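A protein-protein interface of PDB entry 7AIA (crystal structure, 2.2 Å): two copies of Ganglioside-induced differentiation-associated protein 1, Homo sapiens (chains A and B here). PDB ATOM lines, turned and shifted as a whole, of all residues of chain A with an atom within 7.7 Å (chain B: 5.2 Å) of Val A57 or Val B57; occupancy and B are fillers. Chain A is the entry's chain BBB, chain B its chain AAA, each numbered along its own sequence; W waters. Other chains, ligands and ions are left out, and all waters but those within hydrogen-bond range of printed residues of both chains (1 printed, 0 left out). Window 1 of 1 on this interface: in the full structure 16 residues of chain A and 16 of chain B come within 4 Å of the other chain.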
ATOM      1  N   ILE A   5      32.819   2.060  25.297  1.00  0.00           N
ATOM      2  CA  ILE A   5      32.077   1.701  24.056  1.00  0.00           C
ATOM      3  C   ILE A   5      32.249   2.841  23.047  1.00  0.00           C
ATOM      4  O   ILE A   5      32.053   4.004  23.397  1.00  0.00           O
ATOM      5  CB  ILE A   5      30.604   1.442  24.390  1.00  0.00           C
ATOM      6  CG1 ILE A   5      30.467   0.423  25.528  1.00  0.00           C
ATOM      7  CG2 ILE A   5      29.862   1.019  23.148  1.00  0.00           C
ATOM      8  CD1 ILE A   5      29.049   0.235  26.013  1.00  0.00           C
ATOM      9  N   LEU A   6      32.623   2.511  21.824  1.00  0.00           N
ATOM     10  CA  LEU A   6      32.757   3.490  20.734  1.00  0.00           C
ATOM     11  C   LEU A   6      31.881   3.036  19.587  1.00  0.00           C
ATOM     12  O   LEU A   6      32.058   1.907  19.081  1.00  0.00           O
ATOM     13  CB  LEU A   6      34.211   3.557  20.277  1.00  0.00           C
ATOM     14  CG  LEU A   6      34.491   4.541  19.139  1.00  0.00           C
ATOM     15  CD1 LEU A   6      34.370   5.995  19.567  1.00  0.00           C
ATOM     16  CD2 LEU A   6      35.879   4.294  18.643  1.00  0.00           C
ATOM     17  N   TYR A   7      30.997   3.908  19.155  1.00  0.00           N
ATOM     18  CA  TYR A   7      30.271   3.712  17.880  1.00  0.00           C
ATOM     19  C   TYR A   7      30.859   4.688  16.898  1.00  0.00           C
ATOM     20  O   TYR A   7      31.067   5.836  17.293  1.00  0.00           O
ATOM     21  CB  TYR A   7      28.787   3.960  18.067  1.00  0.00           C
ATOM     22  CG  TYR A   7      28.094   2.919  18.881  1.00  0.00           C
ATOM     23  CD1 TYR A   7      27.992   3.059  20.255  1.00  0.00           C
ATOM     24  CD2 TYR A   7      27.443   1.857  18.263  1.00  0.00           C
ATOM     25  CE1 TYR A   7      27.289   2.120  21.008  1.00  0.00           C
ATOM     26  CE2 TYR A   7      26.716   0.938  19.000  1.00  0.00           C
ATOM     27  CZ  TYR A   7      26.654   1.075  20.377  1.00  0.00           C
ATOM     28  OH  TYR A   7      25.962   0.184  21.118  1.00  0.00           O
ATOM     29  N   HIS A   8      31.187   4.211  15.708  1.00  0.00           N
ATOM     30  CA  HIS A   8      32.018   4.951  14.740  1.00  0.00           C
ATOM     31  C   HIS A   8      31.853   4.361  13.342  1.00  0.00           C
ATOM     32  O   HIS A   8      31.236   3.291  13.196  1.00  0.00           O
ATOM     33  CB  HIS A   8      33.469   4.867  15.186  1.00  0.00           C
ATOM     34  CG  HIS A   8      34.102   3.551  14.886  1.00  0.00           C
ATOM     35  ND1 HIS A   8      34.904   3.341  13.777  1.00  0.00           N
ATOM     36  CD2 HIS A   8      34.027   2.371  15.531  1.00  0.00           C
ATOM     37  CE1 HIS A   8      35.306   2.092  13.768  1.00  0.00           C
ATOM     38  NE2 HIS A   8      34.782   1.477  14.832  1.00  0.00           N
ATOM     39  N   TRP A   9      32.440   5.044  12.370  1.00  0.00           N
ATOM     40  CA  TRP A   9      32.612   4.557  10.983  1.00  0.00           C
ATOM     41  C   TRP A   9      34.096   4.365  10.750  1.00  0.00           C
ATOM     42  O   TRP A   9      34.826   5.370  10.805  1.00  0.00           O
ATOM     43  CB  TRP A   9      32.064   5.539   9.967  1.00  0.00           C
ATOM     44  CG  TRP A   9      30.691   5.995  10.304  1.00  0.00           C
ATOM     45  CD1 TRP A   9      29.531   5.453   9.856  1.00  0.00           C
ATOM     46  CD2 TRP A   9      30.339   7.133  11.111  1.00  0.00           C
ATOM     47  NE1 TRP A   9      28.480   6.131  10.379  1.00  0.00           N
ATOM     48  CE2 TRP A   9      28.938   7.198  11.110  1.00  0.00           C
ATOM     49  CE3 TRP A   9      31.068   8.068  11.849  1.00  0.00           C
ATOM     50  CZ2 TRP A   9      28.237   8.185  11.786  1.00  0.00           C
ATOM     51  CZ3 TRP A   9      30.378   9.036  12.533  1.00  0.00           C
ATOM     52  CH2 TRP A   9      28.986   9.082  12.511  1.00  0.00           C
ATOM     53  N   VAL A  18      40.254   9.100  16.724  1.00  0.00           N
ATOM     54  CA  VAL A  18      39.785   8.560  18.039  1.00  0.00           C
ATOM     55  C   VAL A  18      40.411   7.195  18.252  1.00  0.00           C
ATOM     56  O   VAL A  18      40.937   6.949  19.349  1.00  0.00           O
ATOM     57  CB  VAL A  18      38.261   8.453  18.141  1.00  0.00           C
ATOM     58  CG1 VAL A  18      37.855   7.715  19.403  1.00  0.00           C
ATOM     59  CG2 VAL A  18      37.627   9.819  18.080  1.00  0.00           C
ATOM     60  N   CYS A  29      38.640  -1.144  24.529  1.00  0.00           N
ATOM     61  CA  CYS A  29      37.418  -0.477  24.046  1.00  0.00           C
ATOM     62  C   CYS A  29      36.605  -1.432  23.180  1.00  0.00           C
ATOM     63  O   CYS A  29      37.156  -2.016  22.276  1.00  0.00           O
ATOM     64  CB  CYS A  29      37.778   0.768  23.254  1.00  0.00           C
ATOM     65  SG  CYS A  29      36.329   1.679  22.633  1.00  0.00           S
ATOM     66  N   GLU A  30      35.314  -1.532  23.428  1.00  0.00           N
ATOM     67  CA  GLU A  30      34.349  -2.263  22.554  1.00  0.00           C
ATOM     68  C   GLU A  30      33.978  -1.349  21.376  1.00  0.00           C
ATOM     69  O   GLU A  30      33.325  -0.349  21.592  1.00  0.00           O
ATOM     70  CB  GLU A  30      33.179  -2.661  23.430  1.00  0.00           C
ATOM     71  CG  GLU A  30      32.165  -3.561  22.785  1.00  0.00           C
ATOM     72  CD  GLU A  30      30.926  -3.675  23.676  1.00  0.00           C
ATOM     73  OE1 GLU A  30      29.805  -3.234  23.266  1.00  0.00           O
ATOM     74  OE2 GLU A  30      31.102  -4.154  24.819  1.00  0.00           O
ATOM     75  N   HIS A  32      32.303  -0.480  17.803  1.00  0.00           N
ATOM     76  CA  HIS A  32      31.227  -0.882  16.871  1.00  0.00           C
ATOM     77  C   HIS A  32      31.324  -0.029  15.617  1.00  0.00           C
ATOM     78  O   HIS A  32      31.043   1.181  15.685  1.00  0.00           O
ATOM     79  CB  HIS A  32      29.871  -0.744  17.542  1.00  0.00           C
ATOM     80  CG  HIS A  32      29.709  -1.519  18.796  1.00  0.00           C
ATOM     81  ND1 HIS A  32      29.299  -2.823  18.808  1.00  0.00           N
ATOM     82  CD2 HIS A  32      29.853  -1.159  20.092  1.00  0.00           C
ATOM     83  CE1 HIS A  32      29.151  -3.213  20.062  1.00  0.00           C
ATOM     84  NE2 HIS A  32      29.457  -2.209  20.859  1.00  0.00           N
ATOM     85  N   GLU A  54      27.694  13.718  10.700  1.00  0.00           N
ATOM     86  CA  GLU A  54      27.551  12.948  11.963  1.00  0.00           C
ATOM     87  C   GLU A  54      28.922  12.578  12.560  1.00  0.00           C
ATOM     88  O   GLU A  54      29.924  12.372  11.813  1.00  0.00           O
ATOM     89  CB  GLU A  54      26.769  11.651  11.726  1.00  0.00           C
ATOM     90  CG  GLU A  54      25.297  11.875  11.398  1.00  0.00           C
ATOM     91  CD  GLU A  54      24.593  10.603  10.907  1.00  0.00           C
ATOM     92  OE1 GLU A  54      23.502  10.697  10.327  1.00  0.00           O
ATOM     93  OE2 GLU A  54      25.129   9.514  11.143  1.00  0.00           O
ATOM     94  N   VAL A  55      28.931  12.407  13.882  1.00  0.00           N
ATOM     95  CA  VAL A  55      30.169  12.221  14.666  1.00  0.00           C
ATOM     96  C   VAL A  55      30.209  10.842  15.337  1.00  0.00           C
ATOM     97  O   VAL A  55      29.205  10.198  15.573  1.00  0.00           O
ATOM     98  CB  VAL A  55      30.237  13.413  15.619  1.00  0.00           C
ATOM     99  CG1 VAL A  55      30.298  14.729  14.830  1.00  0.00           C
ATOM    100  CG2 VAL A  55      29.067  13.446  16.574  1.00  0.00           C
ATOM    101  N   PRO A  56      31.396  10.301  15.657  1.00  0.00           N
ATOM    102  CA  PRO A  56      31.479   9.138  16.523  1.00  0.00           C
ATOM    103  C   PRO A  56      31.058   9.519  17.960  1.00  0.00           C
ATOM    104  O   PRO A  56      30.929  10.713  18.312  1.00  0.00           O
ATOM    105  CB  PRO A  56      32.957   8.750  16.504  1.00  0.00           C
ATOM    106  CG  PRO A  56      33.657  10.045  16.231  1.00  0.00           C
ATOM    107  CD  PRO A  56      32.715  10.864  15.376  1.00  0.00           C
ATOM    108  N   VAL A  57      30.778   8.495  18.747  1.00  0.00           N
ATOM    109  CA  VAL A  57      30.262   8.696  20.128  1.00  0.00           C
ATOM    110  C   VAL A  57      30.934   7.653  21.043  1.00  0.00           C
ATOM    111  O   VAL A  57      31.061   6.475  20.668  1.00  0.00           O
ATOM    112  CB  VAL A  57      28.724   8.692  20.220  1.00  0.00           C
ATOM    113  CG1 VAL A  57      28.158   7.386  19.765  1.00  0.00           C
ATOM    114  CG2 VAL A  57      28.275   8.907  21.648  1.00  0.00           C
ATOM    115  N   LEU A  58      31.384   8.114  22.192  1.00  0.00           N
ATOM    116  CA  LEU A  58      31.975   7.261  23.239  1.00  0.00           C
ATOM    117  C   LEU A  58      30.995   7.191  24.412  1.00  0.00           C
ATOM    118  O   LEU A  58      30.464   8.248  24.820  1.00  0.00           O
ATOM    119  CB  LEU A  58      33.309   7.853  23.696  1.00  0.00           C
ATOM    120  CG  LEU A  58      34.055   6.957  24.684  1.00  0.00           C
ATOM    121  CD1 LEU A  58      34.843   5.939  23.923  1.00  0.00           C
ATOM    122  CD2 LEU A  58      34.940   7.764  25.601  1.00  0.00           C
ATOM    123  N   ILE A  59      30.718   5.984  24.882  1.00  0.00           N
ATOM    124  CA  ILE A  59      29.983   5.762  26.146  1.00  0.00           C
ATOM    125  C   ILE A  59      30.943   5.133  27.169  1.00  0.00           C
ATOM    126  O   ILE A  59      31.585   4.090  26.885  1.00  0.00           O
ATOM    127  CB  ILE A  59      28.719   4.926  25.915  1.00  0.00           C
ATOM    128  CG1 ILE A  59      27.737   5.597  24.948  1.00  0.00           C
ATOM    129  CG2 ILE A  59      28.036   4.710  27.249  1.00  0.00           C
ATOM    130  CD1 ILE A  59      27.738   5.012  23.638  1.00  0.00           C
ATOM    131  N   HIS A  60      31.038   5.749  28.335  1.00  0.00           N
ATOM    132  CA  HIS A  60      31.947   5.310  29.414  1.00  0.00           C
ATOM    133  C   HIS A  60      31.251   5.510  30.739  1.00  0.00           C
ATOM    134  O   HIS A  60      31.209   6.637  31.223  1.00  0.00           O
ATOM    135  CB  HIS A  60      33.293   6.054  29.328  1.00  0.00           C
ATOM    136  CG  HIS A  60      34.242   5.627  30.390  1.00  0.00           C
ATOM    137  ND1 HIS A  60      34.846   6.535  31.223  1.00  0.00           N
ATOM    138  CD2 HIS A  60      34.622   4.386  30.800  1.00  0.00           C
ATOM    139  CE1 HIS A  60      35.579   5.867  32.103  1.00  0.00           C
ATOM    140  NE2 HIS A  60      35.467   4.553  31.847  1.00  0.00           N
ATOM    141  N   ASN A  63      28.923   8.563  31.196  1.00  0.00           N
ATOM    142  CA  ASN A  63      29.369   9.682  30.332  1.00  0.00           C
ATOM    143  C   ASN A  63      29.126   9.308  28.876  1.00  0.00           C
ATOM    144  O   ASN A  63      29.537   8.240  28.459  1.00  0.00           O
ATOM    145  CB  ASN A  63      30.850  10.019  30.524  1.00  0.00           C
ATOM    146  CG  ASN A  63      31.140  10.548  31.910  1.00  0.00           C
ATOM    147  OD1 ASN A  63      32.010  10.043  32.605  1.00  0.00           O
ATOM    148  ND2 ASN A  63      30.445  11.560  32.302  1.00  0.00           N
ATOM    149  N   ILE A  64      28.473  10.188  28.145  1.00  0.00           N
ATOM    150  CA  ILE A  64      28.262  10.036  26.687  1.00  0.00           C
ATOM    151  C   ILE A  64      28.969  11.229  26.062  1.00  0.00           C
ATOM    152  O   ILE A  64      28.659  12.357  26.475  1.00  0.00           O
ATOM    153  CB  ILE A  64      26.753   9.979  26.380  1.00  0.00           C
ATOM    154  CG1 ILE A  64      26.111   8.830  27.140  1.00  0.00           C
ATOM    155  CG2 ILE A  64      26.531   9.841  24.900  1.00  0.00           C
ATOM    156  CD1 ILE A  64      24.630   8.772  27.003  1.00  0.00           C
ATOM    157  N   ILE A  65      29.923  10.989  25.180  1.00  0.00           N
ATOM    158  CA  ILE A  65      30.706  12.084  24.551  1.00  0.00           C
ATOM    159  C   ILE A  65      30.663  11.880  23.045  1.00  0.00           C
ATOM    160  O   ILE A  65      31.048  10.799  22.544  1.00  0.00           O
ATOM    161  CB  ILE A  65      32.153  12.167  25.096  1.00  0.00           C
ATOM    162  CG1 ILE A  65      32.197  12.323  26.633  1.00  0.00           C
ATOM    163  CG2 ILE A  65      32.847  13.370  24.469  1.00  0.00           C
ATOM    164  CD1 ILE A  65      32.295  11.030  27.358  1.00  0.00           C
ATOM    165  N   CYS A  66      30.295  12.923  22.344  1.00  0.00           N
ATOM    166  CA  CYS A  66      30.204  12.982  20.870  1.00  0.00           C
ATOM    167  C   CYS A  66      31.343  13.857  20.340  1.00  0.00           C
ATOM    168  O   CYS A  66      31.644  14.889  20.981  1.00  0.00           O
ATOM    169  CB  CYS A  66      28.873  13.587  20.440  1.00  0.00           C
ATOM    170  SG  CYS A  66      27.486  12.583  21.011  1.00  0.00           S
ATOM    171  N   GLU A  67      31.812  13.523  19.143  1.00  0.00           N
ATOM    172  CA  GLU A  67      32.762  14.305  18.311  1.00  0.00           C
ATOM    173  C   GLU A  67      34.183  13.910  18.712  1.00  0.00           C
ATOM    174  O   GLU A  67      34.451  13.740  19.889  1.00  0.00           O
ATOM    175  CB  GLU A  67      32.533  15.814  18.370  1.00  0.00           C
ATOM    176  CG  GLU A  67      31.239  16.255  17.701  1.00  0.00           C
ATOM    177  CD  GLU A  67      30.718  17.681  17.916  1.00  0.00           C
ATOM    178  OE1 GLU A  67      30.024  17.984  18.918  1.00  0.00           O
ATOM    179  OE2 GLU A  67      30.941  18.492  17.032  1.00  0.00           O
ATOM    180  N   ALA A  68      35.068  13.798  17.732  1.00  0.00           N
ATOM    181  CA  ALA A  68      36.426  13.267  17.931  1.00  0.00           C
ATOM    182  C   ALA A  68      37.202  14.151  18.917  1.00  0.00           C
ATOM    183  O   ALA A  68      37.829  13.607  19.828  1.00  0.00           O
ATOM    184  CB  ALA A  68      37.147  13.188  16.623  1.00  0.00           C
ATOM    185  N   ILE A  71      35.842  13.641  22.412  1.00  0.00           N
ATOM    186  CA  ILE A  71      36.093  12.258  22.894  1.00  0.00           C
ATOM    187  C   ILE A  71      37.561  12.182  23.310  1.00  0.00           C
ATOM    188  O   ILE A  71      37.878  11.554  24.324  1.00  0.00           O
ATOM    189  CB  ILE A  71      35.766  11.202  21.820  1.00  0.00           C
ATOM    190  CG1 ILE A  71      34.269  11.097  21.573  1.00  0.00           C
ATOM    191  CG2 ILE A  71      36.380   9.843  22.182  1.00  0.00           C
ATOM    192  CD1 ILE A  71      33.886  10.314  20.319  1.00  0.00           C
ATOM    193  N   ILE B   5      18.841   2.084  19.004  1.00  0.00           N
ATOM    194  CA  ILE B   5      19.574   2.062  20.296  1.00  0.00           C
ATOM    195  C   ILE B   5      19.641   3.503  20.829  1.00  0.00           C
ATOM    196  O   ILE B   5      19.986   4.422  20.078  1.00  0.00           O
ATOM    197  CB  ILE B   5      20.944   1.434  20.117  1.00  0.00           C
ATOM    198  CG1 ILE B   5      20.852   0.076  19.423  1.00  0.00           C
ATOM    199  CG2 ILE B   5      21.625   1.314  21.461  1.00  0.00           C
ATOM    200  CD1 ILE B   5      22.177  -0.551  19.047  1.00  0.00           C
ATOM    201  N   LEU B   6      19.197   3.711  22.059  1.00  0.00           N
ATOM    202  CA  LEU B   6      19.275   5.018  22.734  1.00  0.00           C
ATOM    203  C   LEU B   6      20.114   4.847  23.984  1.00  0.00           C
ATOM    204  O   LEU B   6      19.776   3.993  24.815  1.00  0.00           O
ATOM    205  CB  LEU B   6      17.886   5.523  23.081  1.00  0.00           C
ATOM    206  CG  LEU B   6      17.871   6.877  23.795  1.00  0.00           C
ATOM    207  CD1 LEU B   6      18.139   8.010  22.810  1.00  0.00           C
ATOM    208  CD2 LEU B   6      16.541   7.146  24.466  1.00  0.00           C
ATOM    209  N   TYR B   7      21.169   5.637  24.108  1.00  0.00           N
ATOM    210  CA  TYR B   7      21.901   5.811  25.375  1.00  0.00           C
ATOM    211  C   TYR B   7      21.484   7.165  25.931  1.00  0.00           C
ATOM    212  O   TYR B   7      21.395   8.150  25.145  1.00  0.00           O
ATOM    213  CB  TYR B   7      23.384   5.740  25.149  1.00  0.00           C
ATOM    214  CG  TYR B   7      23.893   4.399  24.730  1.00  0.00           C
ATOM    215  CD1 TYR B   7      23.940   4.027  23.394  1.00  0.00           C
ATOM    216  CD2 TYR B   7      24.362   3.500  25.675  1.00  0.00           C
ATOM    217  CE1 TYR B   7      24.409   2.788  23.025  1.00  0.00           C
ATOM    218  CE2 TYR B   7      24.853   2.259  25.317  1.00  0.00           C
ATOM    219  CZ  TYR B   7      24.881   1.915  23.983  1.00  0.00           C
ATOM    220  OH  TYR B   7      25.460   0.732  23.626  1.00  0.00           O
ATOM    221  N   VAL B  55      24.872  14.952  26.120  1.00  0.00           N
ATOM    222  CA  VAL B  55      23.617  14.711  25.389  1.00  0.00           C
ATOM    223  C   VAL B  55      23.302  13.230  25.249  1.00  0.00           C
ATOM    224  O   VAL B  55      24.170  12.382  25.229  1.00  0.00           O
ATOM    225  CB  VAL B  55      23.768  15.466  24.059  1.00  0.00           C
ATOM    226  CG1 VAL B  55      23.948  16.972  24.318  1.00  0.00           C
ATOM    227  CG2 VAL B  55      24.913  14.937  23.226  1.00  0.00           C
ATOM    228  N   PRO B  56      22.026  12.841  25.109  1.00  0.00           N
ATOM    229  CA  PRO B  56      21.682  11.497  24.653  1.00  0.00           C
ATOM    230  C   PRO B  56      22.088  11.271  23.189  1.00  0.00           C
ATOM    231  O   PRO B  56      22.418  12.203  22.470  1.00  0.00           O
ATOM    232  CB  PRO B  56      20.173  11.422  24.712  1.00  0.00           C
ATOM    233  CG  PRO B  56      19.724  12.840  24.579  1.00  0.00           C
ATOM    234  CD  PRO B  56      20.848  13.698  25.115  1.00  0.00           C
ATOM    235  N   VAL B  57      22.191  10.001  22.835  1.00  0.00           N
ATOM    236  CA  VAL B  57      22.665   9.587  21.499  1.00  0.00           C
ATOM    237  C   VAL B  57      21.802   8.412  21.011  1.00  0.00           C
ATOM    238  O   VAL B  57      21.502   7.481  21.774  1.00  0.00           O
ATOM    239  CB  VAL B  57      24.167   9.302  21.458  1.00  0.00           C
ATOM    240  CG1 VAL B  57      24.542   8.235  22.427  1.00  0.00           C
ATOM    241  CG2 VAL B  57      24.617   8.870  20.069  1.00  0.00           C
ATOM    242  N   LEU B  58      21.392   8.506  19.749  1.00  0.00           N
ATOM    243  CA  LEU B  58      20.617   7.472  19.062  1.00  0.00           C
ATOM    244  C   LEU B  58      21.518   6.826  18.023  1.00  0.00           C
ATOM    245  O   LEU B  58      22.216   7.555  17.307  1.00  0.00           O
ATOM    246  CB  LEU B  58      19.384   8.077  18.401  1.00  0.00           C
ATOM    247  CG  LEU B  58      18.456   7.026  17.766  1.00  0.00           C
ATOM    248  CD1 LEU B  58      17.509   6.483  18.805  1.00  0.00           C
ATOM    249  CD2 LEU B  58      17.651   7.589  16.635  1.00  0.00           C
ATOM    250  N   ILE B  59      21.576   5.491  18.028  1.00  0.00           N
ATOM    251  CA  ILE B  59      22.214   4.701  16.964  1.00  0.00           C
ATOM    252  C   ILE B  59      21.103   3.936  16.207  1.00  0.00           C
ATOM    253  O   ILE B  59      20.304   3.171  16.823  1.00  0.00           O
ATOM    254  CB  ILE B  59      23.309   3.799  17.514  1.00  0.00           C
ATOM    255  CG1 ILE B  59      24.411   4.572  18.244  1.00  0.00           C
ATOM    256  CG2 ILE B  59      23.906   2.986  16.389  1.00  0.00           C
ATOM    257  CD1 ILE B  59      24.329   4.475  19.687  1.00  0.00           C
ATOM    258  N   ILE B  64      24.388   7.799  13.573  1.00  0.00           N
ATOM    259  CA  ILE B  64      24.660   8.177  14.977  1.00  0.00           C
ATOM    260  C   ILE B  64      24.172   9.607  15.105  1.00  0.00           C
ATOM    261  O   ILE B  64      24.644  10.457  14.350  1.00  0.00           O
ATOM    262  CB  ILE B  64      26.154   7.993  15.278  1.00  0.00           C
ATOM    263  CG1 ILE B  64      26.568   6.556  15.015  1.00  0.00           C
ATOM    264  CG2 ILE B  64      26.434   8.357  16.717  1.00  0.00           C
ATOM    265  CD1 ILE B  64      28.036   6.351  14.992  1.00  0.00           C
ATOM    266  N   ILE B  65      23.215   9.850  15.978  1.00  0.00           N
ATOM    267  CA  ILE B  65      22.644  11.193  16.148  1.00  0.00           C
ATOM    268  C   ILE B  65      22.694  11.536  17.634  1.00  0.00           C
ATOM    269  O   ILE B  65      22.136  10.806  18.446  1.00  0.00           O
ATOM    270  CB  ILE B  65      21.210  11.336  15.571  1.00  0.00           C
ATOM    271  CG1 ILE B  65      21.097  10.965  14.097  1.00  0.00           C
ATOM    272  CG2 ILE B  65      20.756  12.775  15.733  1.00  0.00           C
ATOM    273  CD1 ILE B  65      20.782   9.528  13.899  1.00  0.00           C
ATOM    274  N   CYS B  66      23.274  12.688  17.935  1.00  0.00           N
ATOM    275  CA  CYS B  66      23.426  13.243  19.313  1.00  0.00           C
ATOM    276  C   CYS B  66      22.492  14.427  19.465  1.00  0.00           C
ATOM    277  O   CYS B  66      22.320  15.161  18.463  1.00  0.00           O
ATOM    278  CB  CYS B  66      24.868  13.675  19.559  1.00  0.00           C
ATOM    279  SG  CYS B  66      26.047  12.319  19.334  1.00  0.00           S
ATOM    280  N   GLU B  67      22.023  14.639  20.694  1.00  0.00           N
ATOM    281  CA  GLU B  67      21.215  15.806  21.166  1.00  0.00           C
ATOM    282  C   GLU B  67      19.750  15.562  20.863  1.00  0.00           C
ATOM    283  O   GLU B  67      19.429  15.019  19.771  1.00  0.00           O
ATOM    284  CB  GLU B  67      21.676  17.133  20.554  1.00  0.00           C
ATOM    285  CG  GLU B  67      23.031  17.587  21.073  1.00  0.00           C
ATOM    286  CD  GLU B  67      23.779  18.670  20.288  1.00  0.00           C
ATOM    287  OE1 GLU B  67      24.925  18.965  20.708  1.00  0.00           O
ATOM    288  OE2 GLU B  67      23.253  19.237  19.268  1.00  0.00           O
ATOM    289  N   ILE B  71      17.895  14.240  17.447  1.00  0.00           N
ATOM    290  CA  ILE B  71      17.393  12.846  17.513  1.00  0.00           C
ATOM    291  C   ILE B  71      15.916  12.867  17.134  1.00  0.00           C
ATOM    292  O   ILE B  71      15.435  11.976  16.396  1.00  0.00           O
ATOM    293  CB  ILE B  71      17.598  12.251  18.915  1.00  0.00           C
ATOM    294  CG1 ILE B  71      19.067  11.989  19.195  1.00  0.00           C
ATOM    295  CG2 ILE B  71      16.758  10.999  19.121  1.00  0.00           C
ATOM    296  CD1 ILE B  71      19.373  11.643  20.645  1.00  0.00           C
HETATM  297  O   HOH W   1      26.983  13.451  24.759  1.00  0.00           O
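Printed residues of chain B that touch a printed residue of chain A: Tyr B7, Val B55, Val B57, Ile B59, Ile B64 and Cys B66. Hydrophobic or aromatic side chains of chain B within 4 Å of the printed part of chain A: Tyr B7, Val B57, Ile B59 and Ile B64. Of the 23 printed residues of chain A, 9 touch a printed residue of chain B. Printed residues of chain A that touch a printed residue of chain B: Tyr A7, His A8, Trp A9, Glu A54, Val A55, Val A57, Ile A59, Ile A64 and Cys A66. Hydrophobic or aromatic side chains of chain A within 4 Å of the printed part of chain B: Tyr A7, Trp A9, Val A57, Ile A59 and Ile A64. Along chain A the printed residues that touch a printed residue of chain B span positions 7 to 66.
Water W1 bridges O of Ile A64 (2.6 Å) and N of Val B55 (2.9 Å).
N of His A8 sits at hydrogen-bond distance from O of His A32 (3.0 Å). The backbone carbonyl oxygen (O) of Ile B5 is in hydrogen-bond range of the backbone NH (N) of Ile B59. O of Val B57 is in hydrogen-bond range of N of Tyr B7. N of Tyr A7 lies within hydrogen-bond range of O of Val A57. The backbone NH of Ile A59 is in hydrogen-bond range of the backbone carbonyl oxygen of Ile A5, at 2.8 Å.
Among the printed residues, merely in contact across the chains: Tyr A7 with Ile B59, Tyr A7 with Ile B64, His A8 with Ile B64, Trp A9 with Ile B64, Val A55 with Ile B64, Val A57 with Val B57, Val A57 with Ile B64, Ile A59 with Tyr B7, Ile A64 with Tyr B7, Ile A64 with Val B55 and Ile A64 with Val B57.
Tyr A7 touches Ile B59, and with the chains exchanged Ile A59 touches Tyr B7. Tyr A7 touches Ile B64, and with the chains exchanged Ile A64 touches Tyr B7. Val A55 touches Ile B64, and with the chains exchanged Ile A64 touches Val B55. Val A57 touches Ile B64, and with the chains exchanged Ile A64 touches Val B57. Of the 14 pairs that touch across the chains among the printed residues, 11 have their exchanged pair printed and touching as well.
The side-chain hydroxyl (OH) of Tyr B7 lies within hydrogen-bond range of the side-chain hydroxyl (OH) of Tyr A7, 2.6 Å away. The side-chain sulfur (SG) of Cys A66 forms a disulfide with the side-chain sulfur (SG) of Cys B66 (2.2 Å). The backbone NH of Ile B64 lies within hydrogen-bond range of the side-chain carboxylate of Glu A54 (3.1 Å).
Printed residues of chain B within 4 Å of Tyr A7: Tyr B7, Ile B59 and Ile B64. Printed residues of chain B within 4 Å of Glu A54: Ile B64. Of the printed residues of chain B, Val A55 touches Ile B64. Printed residues of chain B within 4 Å of Cys A66: Cys B66. Printed residues of chain A within 4 Å of Ile B64: Tyr A7, His A8, Trp A9, Glu A54, Val A55 and Val A57. The nearest residue of chain B that does not touch Val A57 is Cys B66 (4.6 Å). The nearest printed residue of chain A that does not touch Val B57 is Cys A66 (4.7 Å).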
